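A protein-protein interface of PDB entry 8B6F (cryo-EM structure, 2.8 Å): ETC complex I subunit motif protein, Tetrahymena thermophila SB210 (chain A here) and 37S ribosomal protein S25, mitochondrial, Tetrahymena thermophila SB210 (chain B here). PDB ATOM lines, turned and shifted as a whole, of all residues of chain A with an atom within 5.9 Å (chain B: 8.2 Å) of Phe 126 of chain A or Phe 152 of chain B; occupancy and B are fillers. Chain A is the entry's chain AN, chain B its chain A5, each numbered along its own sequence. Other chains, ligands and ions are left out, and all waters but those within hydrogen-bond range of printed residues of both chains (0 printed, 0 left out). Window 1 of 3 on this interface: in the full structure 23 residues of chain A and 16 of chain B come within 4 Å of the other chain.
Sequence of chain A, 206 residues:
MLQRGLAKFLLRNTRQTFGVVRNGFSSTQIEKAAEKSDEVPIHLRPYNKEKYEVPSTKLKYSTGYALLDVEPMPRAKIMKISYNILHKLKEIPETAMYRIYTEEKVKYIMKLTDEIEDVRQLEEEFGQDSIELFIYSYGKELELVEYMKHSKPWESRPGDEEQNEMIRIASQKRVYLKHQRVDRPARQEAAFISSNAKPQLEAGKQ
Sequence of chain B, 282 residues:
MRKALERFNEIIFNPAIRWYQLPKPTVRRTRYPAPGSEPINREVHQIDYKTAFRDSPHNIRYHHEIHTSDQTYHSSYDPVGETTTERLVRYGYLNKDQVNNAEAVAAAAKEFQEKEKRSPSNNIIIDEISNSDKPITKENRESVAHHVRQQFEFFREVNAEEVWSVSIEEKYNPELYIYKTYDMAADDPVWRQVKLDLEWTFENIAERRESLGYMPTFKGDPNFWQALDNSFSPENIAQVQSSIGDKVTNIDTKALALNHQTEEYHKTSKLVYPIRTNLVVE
The side-chain hydroxyl (OG1) of Thr 113 of chain A is in hydrogen-bond range of the backbone carbonyl oxygen (O) of Ile 109 of chain A (2.9 Å).
The side-chain carboxylate (OE2) of Glu 123 of chain A is in hydrogen-bond range of the backbone NH (N) of Ile 131 of chain A (3.3 Å).
The side-chain carboxylate of Glu 153 of chain B is in salt-bridge range of the guanidinium group of Arg 156 of chain B (3.1 Å).
O of Phe 155 of chain B is in hydrogen-bond range of ND2 of Asn 159 of chain B (2.5 Å).
NH2 of Arg 156 of chain B is in salt-bridge range of OE2 of Glu 157 of chain B (3.6 Å).
Lys 105 of chain A touches Val 148 of chain B.
CG of Lys 105 of chain A touches CE2 of Phe 152 of chain B (3.8 Å).
Tyr 108 of chain A touches Phe 152 of chain B.
Glu 123 of chain A touches Ile 168 of chain B.
CG of Arg 156 of chain B touches O of Glu 124 of chain A (3.6 Å).
Phe 126 of chain A touches Phe 152 of chain B (CE1 to CE1, 3.98 Å).
CE2 of Phe 155 of chain B touches C of Phe 126 of chain A (3.4 Å).
Gly 127 of chain A touches Phe 155 of chain B.
Asn 159 of chain B touches Gln 128 of chain A.
Gln 128 of chain A touches Ile 168 of chain B.
Of the printed residues of chain B, Lys 105 of chain A touches Val 148 (3.9 Å) and Phe 152 (3.8 Å).
Thr 113 of chain A touches none of the printed residues of chain B.
Printed residues of chain B within 4 Å of Glu 124 of chain A: Arg 156 (3.6 Å).
Of the printed residues of chain B, Glu 125 of chain A touches Arg 156 (3.3 Å).
Phe 126 of chain A touches just these residues of chain B: Phe 152 (3.98 Å) and Phe 155 (3.4 Å).
Of the printed residues of chain B, Gln 128 of chain A touches Asn 159 and Ile 168.
Gln 150 of chain B touches none of the printed residues of chain A.
Of chain A, only Lys 105 (3.8 Å), Tyr 108 (3.3 Å), Ile 109 (3.5 Å) and Phe 126 (3.98 Å) come within 4 Å of Phe 152 of chain B.
Printed residues of chain A within 4 Å of Phe 155 of chain B: Phe 126 and Gly 127.
The nearest residue of chain A that does not touch Phe 152 of chain B is Glu 125 of chain A (5.0 Å).
Of the 17 printed residues of chain A, 9 touch a printed residue of chain B.
Among the printed residues, Asp or Glu carboxylates within 4 Å of a Lys or Arg side-chain nitrogen of the other chain: Glu 125 of chain A with Arg 156 of chain B (3.4 Å).
The side-chain carboxylate (OE1) of Glu 125 of chain A is in salt-bridge range of the guanidinium group (NH1) of Arg 156 of chain B, 3.4 Å away.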
ATOM      1  N   ILE A  78     -25.176 -17.870 -19.847  1.00  0.00           N
ATOM      2  CA  ILE A  78     -23.796 -17.467 -20.100  1.00  0.00           C
ATOM      3  C   ILE A  78     -23.240 -18.227 -21.295  1.00  0.00           C
ATOM      4  O   ILE A  78     -22.562 -17.653 -22.154  1.00  0.00           O
ATOM      5  CB  ILE A  78     -22.926 -17.678 -18.847  1.00  0.00           C
ATOM      6  CG1 ILE A  78     -23.400 -16.767 -17.717  1.00  0.00           C
ATOM      7  CG2 ILE A  78     -21.461 -17.401 -19.166  1.00  0.00           C
ATOM      8  CD1 ILE A  78     -22.714 -17.006 -16.387  1.00  0.00           C
ATOM      9  N   LYS A 105     -11.487 -13.006 -23.330  1.00  0.00           N
ATOM     10  CA  LYS A 105     -12.418 -12.806 -22.226  1.00  0.00           C
ATOM     11  C   LYS A 105     -13.527 -13.849 -22.244  1.00  0.00           C
ATOM     12  O   LYS A 105     -13.893 -14.396 -21.198  1.00  0.00           O
ATOM     13  CB  LYS A 105     -13.005 -11.397 -22.296  1.00  0.00           C
ATOM     14  CG  LYS A 105     -13.963 -11.072 -21.163  1.00  0.00           C
ATOM     15  CD  LYS A 105     -14.281  -9.586 -21.110  1.00  0.00           C
ATOM     16  CE  LYS A 105     -14.948  -9.109 -22.390  1.00  0.00           C
ATOM     17  NZ  LYS A 105     -15.337  -7.676 -22.307  1.00  0.00           N
ATOM     18  N   TYR A 108     -12.169 -17.221 -21.090  1.00  0.00           N
ATOM     19  CA  TYR A 108     -11.997 -17.254 -19.644  1.00  0.00           C
ATOM     20  C   TYR A 108     -13.337 -17.435 -18.941  1.00  0.00           C
ATOM     21  O   TYR A 108     -13.468 -18.256 -18.028  1.00  0.00           O
ATOM     22  CB  TYR A 108     -11.307 -15.973 -19.175  1.00  0.00           C
ATOM     23  CG  TYR A 108     -11.173 -15.866 -17.674  1.00  0.00           C
ATOM     24  CD1 TYR A 108     -12.190 -15.318 -16.904  1.00  0.00           C
ATOM     25  CD2 TYR A 108     -10.024 -16.298 -17.030  1.00  0.00           C
ATOM     26  CE1 TYR A 108     -12.071 -15.214 -15.534  1.00  0.00           C
ATOM     27  CE2 TYR A 108      -9.894 -16.198 -15.659  1.00  0.00           C
ATOM     28  CZ  TYR A 108     -10.922 -15.655 -14.918  1.00  0.00           C
ATOM     29  OH  TYR A 108     -10.801 -15.551 -13.553  1.00  0.00           O
ATOM     30  N   ILE A 109     -14.348 -16.665 -19.352  1.00  0.00           N
ATOM     31  CA  ILE A 109     -15.653 -16.740 -18.699  1.00  0.00           C
ATOM     32  C   ILE A 109     -16.260 -18.126 -18.879  1.00  0.00           C
ATOM     33  O   ILE A 109     -16.809 -18.707 -17.936  1.00  0.00           O
ATOM     34  CB  ILE A 109     -16.585 -15.638 -19.236  1.00  0.00           C
ATOM     35  CG1 ILE A 109     -16.054 -14.260 -18.838  1.00  0.00           C
ATOM     36  CG2 ILE A 109     -18.007 -15.828 -18.711  1.00  0.00           C
ATOM     37  CD1 ILE A 109     -16.789 -13.103 -19.485  1.00  0.00           C
ATOM     38  N   LEU A 112     -14.474 -20.714 -16.661  1.00  0.00           N
ATOM     39  CA  LEU A 112     -14.851 -20.569 -15.260  1.00  0.00           C
ATOM     40  C   LEU A 112     -16.267 -21.074 -15.016  1.00  0.00           C
ATOM     41  O   LEU A 112     -16.529 -21.753 -14.016  1.00  0.00           O
ATOM     42  CB  LEU A 112     -14.718 -19.108 -14.832  1.00  0.00           C
ATOM     43  CG  LEU A 112     -14.853 -18.839 -13.332  1.00  0.00           C
ATOM     44  CD1 LEU A 112     -13.776 -19.565 -12.541  1.00  0.00           C
ATOM     45  CD2 LEU A 112     -14.794 -17.356 -13.058  1.00  0.00           C
ATOM     46  N   THR A 113     -17.199 -20.745 -15.913  1.00  0.00           N
ATOM     47  CA  THR A 113     -18.581 -21.179 -15.736  1.00  0.00           C
ATOM     48  C   THR A 113     -18.697 -22.695 -15.807  1.00  0.00           C
ATOM     49  O   THR A 113     -19.422 -23.308 -15.016  1.00  0.00           O
ATOM     50  CB  THR A 113     -19.475 -20.525 -16.789  1.00  0.00           C
ATOM     51  OG1 THR A 113     -19.416 -19.102 -16.646  1.00  0.00           O
ATOM     52  CG2 THR A 113     -20.922 -20.988 -16.641  1.00  0.00           C
ATOM     53  N   GLN A 121     -20.951 -19.908  -5.808  1.00  0.00           N
ATOM     54  CA  GLN A 121     -19.518 -19.811  -6.064  1.00  0.00           C
ATOM     55  C   GLN A 121     -19.239 -18.998  -7.319  1.00  0.00           C
ATOM     56  O   GLN A 121     -18.303 -18.192  -7.352  1.00  0.00           O
ATOM     57  CB  GLN A 121     -18.908 -21.206  -6.187  1.00  0.00           C
ATOM     58  CG  GLN A 121     -18.960 -22.012  -4.905  1.00  0.00           C
ATOM     59  CD  GLN A 121     -18.420 -23.414  -5.084  1.00  0.00           C
ATOM     60  OE1 GLN A 121     -17.883 -23.755  -6.137  1.00  0.00           O
ATOM     61  NE2 GLN A 121     -18.560 -24.238  -4.051  1.00  0.00           N
ATOM     62  N   LEU A 122     -20.041 -19.197  -8.366  1.00  0.00           N
ATOM     63  CA  LEU A 122     -19.857 -18.427  -9.591  1.00  0.00           C
ATOM     64  C   LEU A 122     -20.071 -16.941  -9.340  1.00  0.00           C
ATOM     65  O   LEU A 122     -19.324 -16.101  -9.855  1.00  0.00           O
ATOM     66  CB  LEU A 122     -20.809 -18.935 -10.676  1.00  0.00           C
ATOM     67  CG  LEU A 122     -20.606 -18.354 -12.078  1.00  0.00           C
ATOM     68  CD1 LEU A 122     -19.216 -18.672 -12.603  1.00  0.00           C
ATOM     69  CD2 LEU A 122     -21.666 -18.871 -13.033  1.00  0.00           C
ATOM     70  N   GLU A 123     -21.085 -16.596  -8.543  1.00  0.00           N
ATOM     71  CA  GLU A 123     -21.316 -15.196  -8.202  1.00  0.00           C
ATOM     72  C   GLU A 123     -20.157 -14.627  -7.397  1.00  0.00           C
ATOM     73  O   GLU A 123     -19.734 -13.487  -7.623  1.00  0.00           O
ATOM     74  CB  GLU A 123     -22.624 -15.051  -7.428  1.00  0.00           C
ATOM     75  CG  GLU A 123     -23.861 -15.285  -8.272  1.00  0.00           C
ATOM     76  CD  GLU A 123     -25.138 -15.154  -7.472  1.00  0.00           C
ATOM     77  OE1 GLU A 123     -25.052 -14.929  -6.247  1.00  0.00           O
ATOM     78  OE2 GLU A 123     -26.230 -15.275  -8.065  1.00  0.00           O
ATOM     79  N   GLU A 124     -19.631 -15.403  -6.450  1.00  0.00           N
ATOM     80  CA  GLU A 124     -18.484 -14.941  -5.677  1.00  0.00           C
ATOM     81  C   GLU A 124     -17.289 -14.677  -6.582  1.00  0.00           C
ATOM     82  O   GLU A 124     -16.538 -13.718  -6.367  1.00  0.00           O
ATOM     83  CB  GLU A 124     -18.132 -15.970  -4.602  1.00  0.00           C
ATOM     84  CG  GLU A 124     -19.165 -16.071  -3.494  1.00  0.00           C
ATOM     85  CD  GLU A 124     -18.839 -17.159  -2.492  1.00  0.00           C
ATOM     86  OE1 GLU A 124     -17.739 -17.741  -2.585  1.00  0.00           O
ATOM     87  OE2 GLU A 124     -19.682 -17.435  -1.615  1.00  0.00           O
ATOM     88  N   GLU A 125     -17.086 -15.524  -7.592  1.00  0.00           N
ATOM     89  CA  GLU A 125     -16.019 -15.279  -8.556  1.00  0.00           C
ATOM     90  C   GLU A 125     -16.277 -14.000  -9.343  1.00  0.00           C
ATOM     91  O   GLU A 125     -15.388 -13.154  -9.487  1.00  0.00           O
ATOM     92  CB  GLU A 125     -15.891 -16.471  -9.502  1.00  0.00           C
ATOM     93  CG  GLU A 125     -15.229 -17.686  -8.883  1.00  0.00           C
ATOM     94  CD  GLU A 125     -13.758 -17.471  -8.595  1.00  0.00           C
ATOM     95  OE1 GLU A 125     -13.206 -16.448  -9.049  1.00  0.00           O
ATOM     96  OE2 GLU A 125     -13.153 -18.327  -7.916  1.00  0.00           O
ATOM     97  N   PHE A 126     -17.496 -13.843  -9.864  1.00  0.00           N
ATOM     98  CA  PHE A 126     -17.870 -12.655 -10.634  1.00  0.00           C
ATOM     99  C   PHE A 126     -18.360 -11.586  -9.665  1.00  0.00           C
ATOM    100  O   PHE A 126     -19.557 -11.348  -9.497  1.00  0.00           O
ATOM    101  CB  PHE A 126     -18.929 -12.998 -11.675  1.00  0.00           C
ATOM    102  CG  PHE A 126     -18.442 -13.908 -12.768  1.00  0.00           C
ATOM    103  CD1 PHE A 126     -17.159 -13.787 -13.276  1.00  0.00           C
ATOM    104  CD2 PHE A 126     -19.272 -14.885 -13.288  1.00  0.00           C
ATOM    105  CE1 PHE A 126     -16.716 -14.619 -14.282  1.00  0.00           C
ATOM    106  CE2 PHE A 126     -18.834 -15.721 -14.294  1.00  0.00           C
ATOM    107  CZ  PHE A 126     -17.555 -15.589 -14.790  1.00  0.00           C
ATOM    108  N   GLY A 127     -17.404 -10.921  -9.026  1.00  0.00           N
ATOM    109  CA  GLY A 127     -17.760  -9.950  -8.015  1.00  0.00           C
ATOM    110  C   GLY A 127     -18.473 -10.627  -6.861  1.00  0.00           C
ATOM    111  O   GLY A 127     -18.191 -11.773  -6.501  1.00  0.00           O
ATOM    112  N   GLN A 128     -19.412  -9.898  -6.260  1.00  0.00           N
ATOM    113  CA  GLN A 128     -20.276 -10.467  -5.233  1.00  0.00           C
ATOM    114  C   GLN A 128     -21.707  -9.967  -5.386  1.00  0.00           C
ATOM    115  O   GLN A 128     -22.441  -9.857  -4.397  1.00  0.00           O
ATOM    116  CB  GLN A 128     -19.744 -10.158  -3.832  1.00  0.00           C
ATOM    117  CG  GLN A 128     -18.460 -10.902  -3.494  1.00  0.00           C
ATOM    118  CD  GLN A 128     -18.002 -10.661  -2.072  1.00  0.00           C
ATOM    119  OE1 GLN A 128     -18.364  -9.662  -1.452  1.00  0.00           O
ATOM    120  NE2 GLN A 128     -17.206 -11.582  -1.544  1.00  0.00           N
ATOM    121  N   ASP A 129     -22.116  -9.658  -6.612  1.00  0.00           N
ATOM    122  CA  ASP A 129     -23.451  -9.166  -6.901  1.00  0.00           C
ATOM    123  C   ASP A 129     -24.290 -10.286  -7.515  1.00  0.00           C
ATOM    124  O   ASP A 129     -23.823 -11.407  -7.724  1.00  0.00           O
ATOM    125  CB  ASP A 129     -23.374  -7.952  -7.829  1.00  0.00           C
ATOM    126  CG  ASP A 129     -24.589  -7.053  -7.715  1.00  0.00           C
ATOM    127  OD1 ASP A 129     -25.664  -7.550  -7.325  1.00  0.00           O
ATOM    128  OD2 ASP A 129     -24.468  -5.846  -8.016  1.00  0.00           O
ATOM    129  N   ILE A 131     -26.101 -12.699 -10.043  1.00  0.00           N
ATOM    130  CA  ILE A 131     -25.684 -13.222 -11.339  1.00  0.00           C
ATOM    131  C   ILE A 131     -26.513 -12.606 -12.455  1.00  0.00           C
ATOM    132  O   ILE A 131     -26.049 -12.497 -13.595  1.00  0.00           O
ATOM    133  CB  ILE A 131     -25.780 -14.760 -11.347  1.00  0.00           C
ATOM    134  CG1 ILE A 131     -25.003 -15.347 -12.526  1.00  0.00           C
ATOM    135  CG2 ILE A 131     -27.235 -15.217 -11.399  1.00  0.00           C
ATOM    136  CD1 ILE A 131     -23.499 -15.244 -12.384  1.00  0.00           C
ATOM    137  N   PHE A 134     -24.854  -9.535 -13.873  1.00  0.00           N
ATOM    138  CA  PHE A 134     -23.740  -9.926 -14.729  1.00  0.00           C
ATOM    139  C   PHE A 134     -24.238 -10.438 -16.075  1.00  0.00           C
ATOM    140  O   PHE A 134     -23.649 -10.137 -17.120  1.00  0.00           O
ATOM    141  CB  PHE A 134     -22.893 -10.989 -14.029  1.00  0.00           C
ATOM    142  CG  PHE A 134     -21.707 -11.442 -14.829  1.00  0.00           C
ATOM    143  CD1 PHE A 134     -20.502 -10.767 -14.746  1.00  0.00           C
ATOM    144  CD2 PHE A 134     -21.794 -12.547 -15.661  1.00  0.00           C
ATOM    145  CE1 PHE A 134     -19.406 -11.180 -15.480  1.00  0.00           C
ATOM    146  CE2 PHE A 134     -20.703 -12.966 -16.397  1.00  0.00           C
ATOM    147  CZ  PHE A 134     -19.508 -12.281 -16.305  1.00  0.00           C
ATOM    148  N   ALA B 145      -4.269 -12.688 -22.742  1.00  0.00           N
ATOM    149  CA  ALA B 145      -4.823 -13.623 -21.770  1.00  0.00           C
ATOM    150  C   ALA B 145      -4.380 -13.275 -20.355  1.00  0.00           C
ATOM    151  O   ALA B 145      -5.180 -13.332 -19.415  1.00  0.00           O
ATOM    152  CB  ALA B 145      -4.412 -15.052 -22.122  1.00  0.00           C
ATOM    153  N   HIS B 146      -3.108 -12.912 -20.186  1.00  0.00           N
ATOM    154  CA  HIS B 146      -2.624 -12.526 -18.867  1.00  0.00           C
ATOM    155  C   HIS B 146      -3.358 -11.295 -18.353  1.00  0.00           C
ATOM    156  O   HIS B 146      -3.734 -11.232 -17.178  1.00  0.00           O
ATOM    157  CB  HIS B 146      -1.118 -12.269 -18.916  1.00  0.00           C
ATOM    158  CG  HIS B 146      -0.535 -11.859 -17.599  1.00  0.00           C
ATOM    159  ND1 HIS B 146      -0.489 -10.546 -17.182  1.00  0.00           N
ATOM    160  CD2 HIS B 146       0.025 -12.589 -16.606  1.00  0.00           C
ATOM    161  CE1 HIS B 146       0.075 -10.485 -15.989  1.00  0.00           C
ATOM    162  NE2 HIS B 146       0.395 -11.710 -15.616  1.00  0.00           N
ATOM    163  N   HIS B 147      -3.565 -10.303 -19.220  1.00  0.00           N
ATOM    164  CA  HIS B 147      -4.286  -9.106 -18.807  1.00  0.00           C
ATOM    165  C   HIS B 147      -5.733  -9.425 -18.456  1.00  0.00           C
ATOM    166  O   HIS B 147      -6.289  -8.856 -17.510  1.00  0.00           O
ATOM    167  CB  HIS B 147      -4.227  -8.049 -19.907  1.00  0.00           C
ATOM    168  CG  HIS B 147      -5.235  -6.959 -19.739  1.00  0.00           C
ATOM    169  ND1 HIS B 147      -6.446  -6.960 -20.398  1.00  0.00           N
ATOM    170  CD2 HIS B 147      -5.227  -5.846 -18.970  1.00  0.00           C
ATOM    171  CE1 HIS B 147      -7.135  -5.889 -20.049  1.00  0.00           C
ATOM    172  NE2 HIS B 147      -6.418  -5.196 -19.181  1.00  0.00           N
ATOM    173  N   VAL B 148      -6.361 -10.333 -19.204  1.00  0.00           N
ATOM    174  CA  VAL B 148      -7.733 -10.723 -18.892  1.00  0.00           C
ATOM    175  C   VAL B 148      -7.795 -11.385 -17.522  1.00  0.00           C
ATOM    176  O   VAL B 148      -8.687 -11.093 -16.716  1.00  0.00           O
ATOM    177  CB  VAL B 148      -8.290 -11.642 -19.995  1.00  0.00           C
ATOM    178  CG1 VAL B 148      -9.606 -12.285 -19.560  1.00  0.00           C
ATOM    179  CG2 VAL B 148      -8.491 -10.861 -21.281  1.00  0.00           C
ATOM    180  N   ARG B 149      -6.858 -12.290 -17.237  1.00  0.00           N
ATOM    181  CA  ARG B 149      -6.834 -12.927 -15.924  1.00  0.00           C
ATOM    182  C   ARG B 149      -6.625 -11.895 -14.823  1.00  0.00           C
ATOM    183  O   ARG B 149      -7.278 -11.952 -13.776  1.00  0.00           O
ATOM    184  CB  ARG B 149      -5.745 -13.999 -15.879  1.00  0.00           C
ATOM    185  CG  ARG B 149      -6.092 -15.239 -16.684  1.00  0.00           C
ATOM    186  CD  ARG B 149      -5.090 -16.363 -16.468  1.00  0.00           C
ATOM    187  NE  ARG B 149      -3.896 -16.211 -17.292  1.00  0.00           N
ATOM    188  CZ  ARG B 149      -2.769 -15.634 -16.897  1.00  0.00           C
ATOM    189  NH1 ARG B 149      -2.637 -15.122 -15.684  1.00  0.00           N
ATOM    190  NH2 ARG B 149      -1.744 -15.571 -17.743  1.00  0.00           N
ATOM    191  N   GLN B 150      -5.716 -10.945 -15.043  1.00  0.00           N
ATOM    192  CA  GLN B 150      -5.494  -9.888 -14.062  1.00  0.00           C
ATOM    193  C   GLN B 150      -6.745  -9.041 -13.873  1.00  0.00           C
ATOM    194  O   GLN B 150      -7.081  -8.658 -12.747  1.00  0.00           O
ATOM    195  CB  GLN B 150      -4.318  -9.013 -14.495  1.00  0.00           C
ATOM    196  CG  GLN B 150      -4.028  -7.856 -13.554  1.00  0.00           C
ATOM    197  CD  GLN B 150      -2.855  -7.020 -14.015  1.00  0.00           C
ATOM    198  OE1 GLN B 150      -2.228  -7.320 -15.029  1.00  0.00           O
ATOM    199  NE2 GLN B 150      -2.553  -5.962 -13.270  1.00  0.00           N
ATOM    200  N   GLN B 151      -7.441  -8.730 -14.967  1.00  0.00           N
ATOM    201  CA  GLN B 151      -8.648  -7.917 -14.874  1.00  0.00           C
ATOM    202  C   GLN B 151      -9.730  -8.618 -14.062  1.00  0.00           C
ATOM    203  O   GLN B 151     -10.403  -7.988 -13.240  1.00  0.00           O
ATOM    204  CB  GLN B 151      -9.155  -7.593 -16.277  1.00  0.00           C
ATOM    205  CG  GLN B 151     -10.453  -6.810 -16.313  1.00  0.00           C
ATOM    206  CD  GLN B 151     -10.914  -6.513 -17.728  1.00  0.00           C
ATOM    207  OE1 GLN B 151     -11.375  -5.412 -18.019  1.00  0.00           O
ATOM    208  NE2 GLN B 151     -10.812  -7.503 -18.608  1.00  0.00           N
ATOM    209  N   PHE B 152      -9.921  -9.919 -14.285  1.00  0.00           N
ATOM    210  CA  PHE B 152     -10.931 -10.649 -13.526  1.00  0.00           C
ATOM    211  C   PHE B 152     -10.511 -10.814 -12.072  1.00  0.00           C
ATOM    212  O   PHE B 152     -11.356 -10.791 -11.171  1.00  0.00           O
ATOM    213  CB  PHE B 152     -11.202 -12.004 -14.174  1.00  0.00           C
ATOM    214  CG  PHE B 152     -12.179 -11.938 -15.307  1.00  0.00           C
ATOM    215  CD1 PHE B 152     -13.542 -11.971 -15.063  1.00  0.00           C
ATOM    216  CD2 PHE B 152     -11.740 -11.834 -16.615  1.00  0.00           C
ATOM    217  CE1 PHE B 152     -14.447 -11.906 -16.101  1.00  0.00           C
ATOM    218  CE2 PHE B 152     -12.641 -11.770 -17.659  1.00  0.00           C
ATOM    219  CZ  PHE B 152     -13.996 -11.805 -17.402  1.00  0.00           C
ATOM    220  N   GLU B 153      -9.214 -10.996 -11.823  1.00  0.00           N
ATOM    221  CA  GLU B 153      -8.727 -11.030 -10.448  1.00  0.00           C
ATOM    222  C   GLU B 153      -9.049  -9.725  -9.735  1.00  0.00           C
ATOM    223  O   GLU B 153      -9.535  -9.725  -8.599  1.00  0.00           O
ATOM    224  CB  GLU B 153      -7.221 -11.297 -10.437  1.00  0.00           C
ATOM    225  CG  GLU B 153      -6.576 -11.265  -9.055  1.00  0.00           C
ATOM    226  CD  GLU B 153      -7.082 -12.365  -8.146  1.00  0.00           C
ATOM    227  OE1 GLU B 153      -7.797 -13.262  -8.638  1.00  0.00           O
ATOM    228  OE2 GLU B 153      -6.765 -12.332  -6.938  1.00  0.00           O
ATOM    229  N   PHE B 154      -8.793  -8.597 -10.396  1.00  0.00           N
ATOM    230  CA  PHE B 154      -9.125  -7.305  -9.809  1.00  0.00           C
ATOM    231  C   PHE B 154     -10.626  -7.166  -9.604  1.00  0.00           C
ATOM    232  O   PHE B 154     -11.075  -6.665  -8.567  1.00  0.00           O
ATOM    233  CB  PHE B 154      -8.601  -6.173 -10.691  1.00  0.00           C
ATOM    234  CG  PHE B 154      -9.129  -4.822 -10.315  1.00  0.00           C
ATOM    235  CD1 PHE B 154      -8.555  -4.103  -9.280  1.00  0.00           C
ATOM    236  CD2 PHE B 154     -10.199  -4.268 -10.996  1.00  0.00           C
ATOM    237  CE1 PHE B 154      -9.042  -2.858  -8.931  1.00  0.00           C
ATOM    238  CE2 PHE B 154     -10.690  -3.024 -10.651  1.00  0.00           C
ATOM    239  CZ  PHE B 154     -10.110  -2.318  -9.617  1.00  0.00           C
ATOM    240  N   PHE B 155     -11.420  -7.610 -10.579  1.00  0.00           N
ATOM    241  CA  PHE B 155     -12.869  -7.507 -10.460  1.00  0.00           C
ATOM    242  C   PHE B 155     -13.379  -8.266  -9.242  1.00  0.00           C
ATOM    243  O   PHE B 155     -14.302  -7.808  -8.559  1.00  0.00           O
ATOM    244  CB  PHE B 155     -13.531  -8.024 -11.737  1.00  0.00           C
ATOM    245  CG  PHE B 155     -15.024  -8.123 -11.648  1.00  0.00           C
ATOM    246  CD1 PHE B 155     -15.779  -7.052 -11.201  1.00  0.00           C
ATOM    247  CD2 PHE B 155     -15.677  -9.281 -12.036  1.00  0.00           C
ATOM    248  CE1 PHE B 155     -17.155  -7.138 -11.129  1.00  0.00           C
ATOM    249  CE2 PHE B 155     -17.052  -9.375 -11.964  1.00  0.00           C
ATOM    250  CZ  PHE B 155     -17.792  -8.300 -11.512  1.00  0.00           C
ATOM    251  N   ARG B 156     -12.803  -9.433  -8.960  1.00  0.00           N
ATOM    252  CA  ARG B 156     -13.204 -10.181  -7.774  1.00  0.00           C
ATOM    253  C   ARG B 156     -12.720  -9.495  -6.502  1.00  0.00           C
ATOM    254  O   ARG B 156     -13.483  -9.329  -5.545  1.00  0.00           O
ATOM    255  CB  ARG B 156     -12.674 -11.612  -7.847  1.00  0.00           C
ATOM    256  CG  ARG B 156     -13.167 -12.484  -6.708  1.00  0.00           C
ATOM    257  CD  ARG B 156     -12.771 -13.938  -6.881  1.00  0.00           C
ATOM    258  NE  ARG B 156     -11.349 -14.161  -6.653  1.00  0.00           N
ATOM    259  CZ  ARG B 156     -10.428 -14.225  -7.606  1.00  0.00           C
ATOM    260  NH1 ARG B 156     -10.738 -14.067  -8.883  1.00  0.00           N
ATOM    261  NH2 ARG B 156      -9.163 -14.456  -7.270  1.00  0.00           N
ATOM    262  N   GLU B 157     -11.448  -9.092  -6.473  1.00  0.00           N
ATOM    263  CA  GLU B 157     -10.843  -8.638  -5.225  1.00  0.00           C
ATOM    264  C   GLU B 157     -11.368  -7.270  -4.804  1.00  0.00           C
ATOM    265  O   GLU B 157     -11.543  -7.012  -3.608  1.00  0.00           O
ATOM    266  CB  GLU B 157      -9.322  -8.601  -5.360  1.00  0.00           C
ATOM    267  CG  GLU B 157      -8.682  -9.961  -5.584  1.00  0.00           C
ATOM    268  CD  GLU B 157      -8.876 -10.902  -4.411  1.00  0.00           C
ATOM    269  OE1 GLU B 157      -9.275 -10.432  -3.325  1.00  0.00           O
ATOM    270  OE2 GLU B 157      -8.632 -12.116  -4.575  1.00  0.00           O
ATOM    271  N   VAL B 158     -11.617  -6.376  -5.763  1.00  0.00           N
ATOM    272  CA  VAL B 158     -12.106  -5.044  -5.415  1.00  0.00           C
ATOM    273  C   VAL B 158     -13.480  -5.136  -4.764  1.00  0.00           C
ATOM    274  O   VAL B 158     -13.771  -4.435  -3.788  1.00  0.00           O
ATOM    275  CB  VAL B 158     -12.122  -4.130  -6.656  1.00  0.00           C
ATOM    276  CG1 VAL B 158     -13.150  -4.598  -7.680  1.00  0.00           C
ATOM    277  CG2 VAL B 158     -12.391  -2.690  -6.247  1.00  0.00           C
ATOM    278  N   ASN B 159     -14.348  -5.993  -5.299  1.00  0.00           N
ATOM    279  CA  ASN B 159     -15.651  -6.211  -4.681  1.00  0.00           C
ATOM    280  C   ASN B 159     -15.516  -6.938  -3.350  1.00  0.00           C
ATOM    281  O   ASN B 159     -16.271  -6.668  -2.411  1.00  0.00           O
ATOM    282  CB  ASN B 159     -16.554  -6.993  -5.632  1.00  0.00           C
ATOM    283  CG  ASN B 159     -16.933  -6.194  -6.860  1.00  0.00           C
ATOM    284  OD1 ASN B 159     -17.953  -5.506  -6.875  1.00  0.00           O
ATOM    285  ND2 ASN B 159     -16.114  -6.281  -7.900  1.00  0.00           N
ATOM    286  N   ILE B 168     -22.342 -10.957  -0.606  1.00  0.00           N
ATOM    287  CA  ILE B 168     -23.084 -12.131  -1.056  1.00  0.00           C
ATOM    288  C   ILE B 168     -23.958 -12.670   0.066  1.00  0.00           C
ATOM    289  O   ILE B 168     -25.054 -13.185  -0.181  1.00  0.00           O
ATOM    290  CB  ILE B 168     -22.116 -13.204  -1.593  1.00  0.00           C
ATOM    291  CG1 ILE B 168     -22.884 -14.301  -2.336  1.00  0.00           C
ATOM    292  CG2 ILE B 168     -21.296 -13.814  -0.465  1.00  0.00           C
ATOM    293  CD1 ILE B 168     -23.526 -13.843  -3.630  1.00  0.00           C
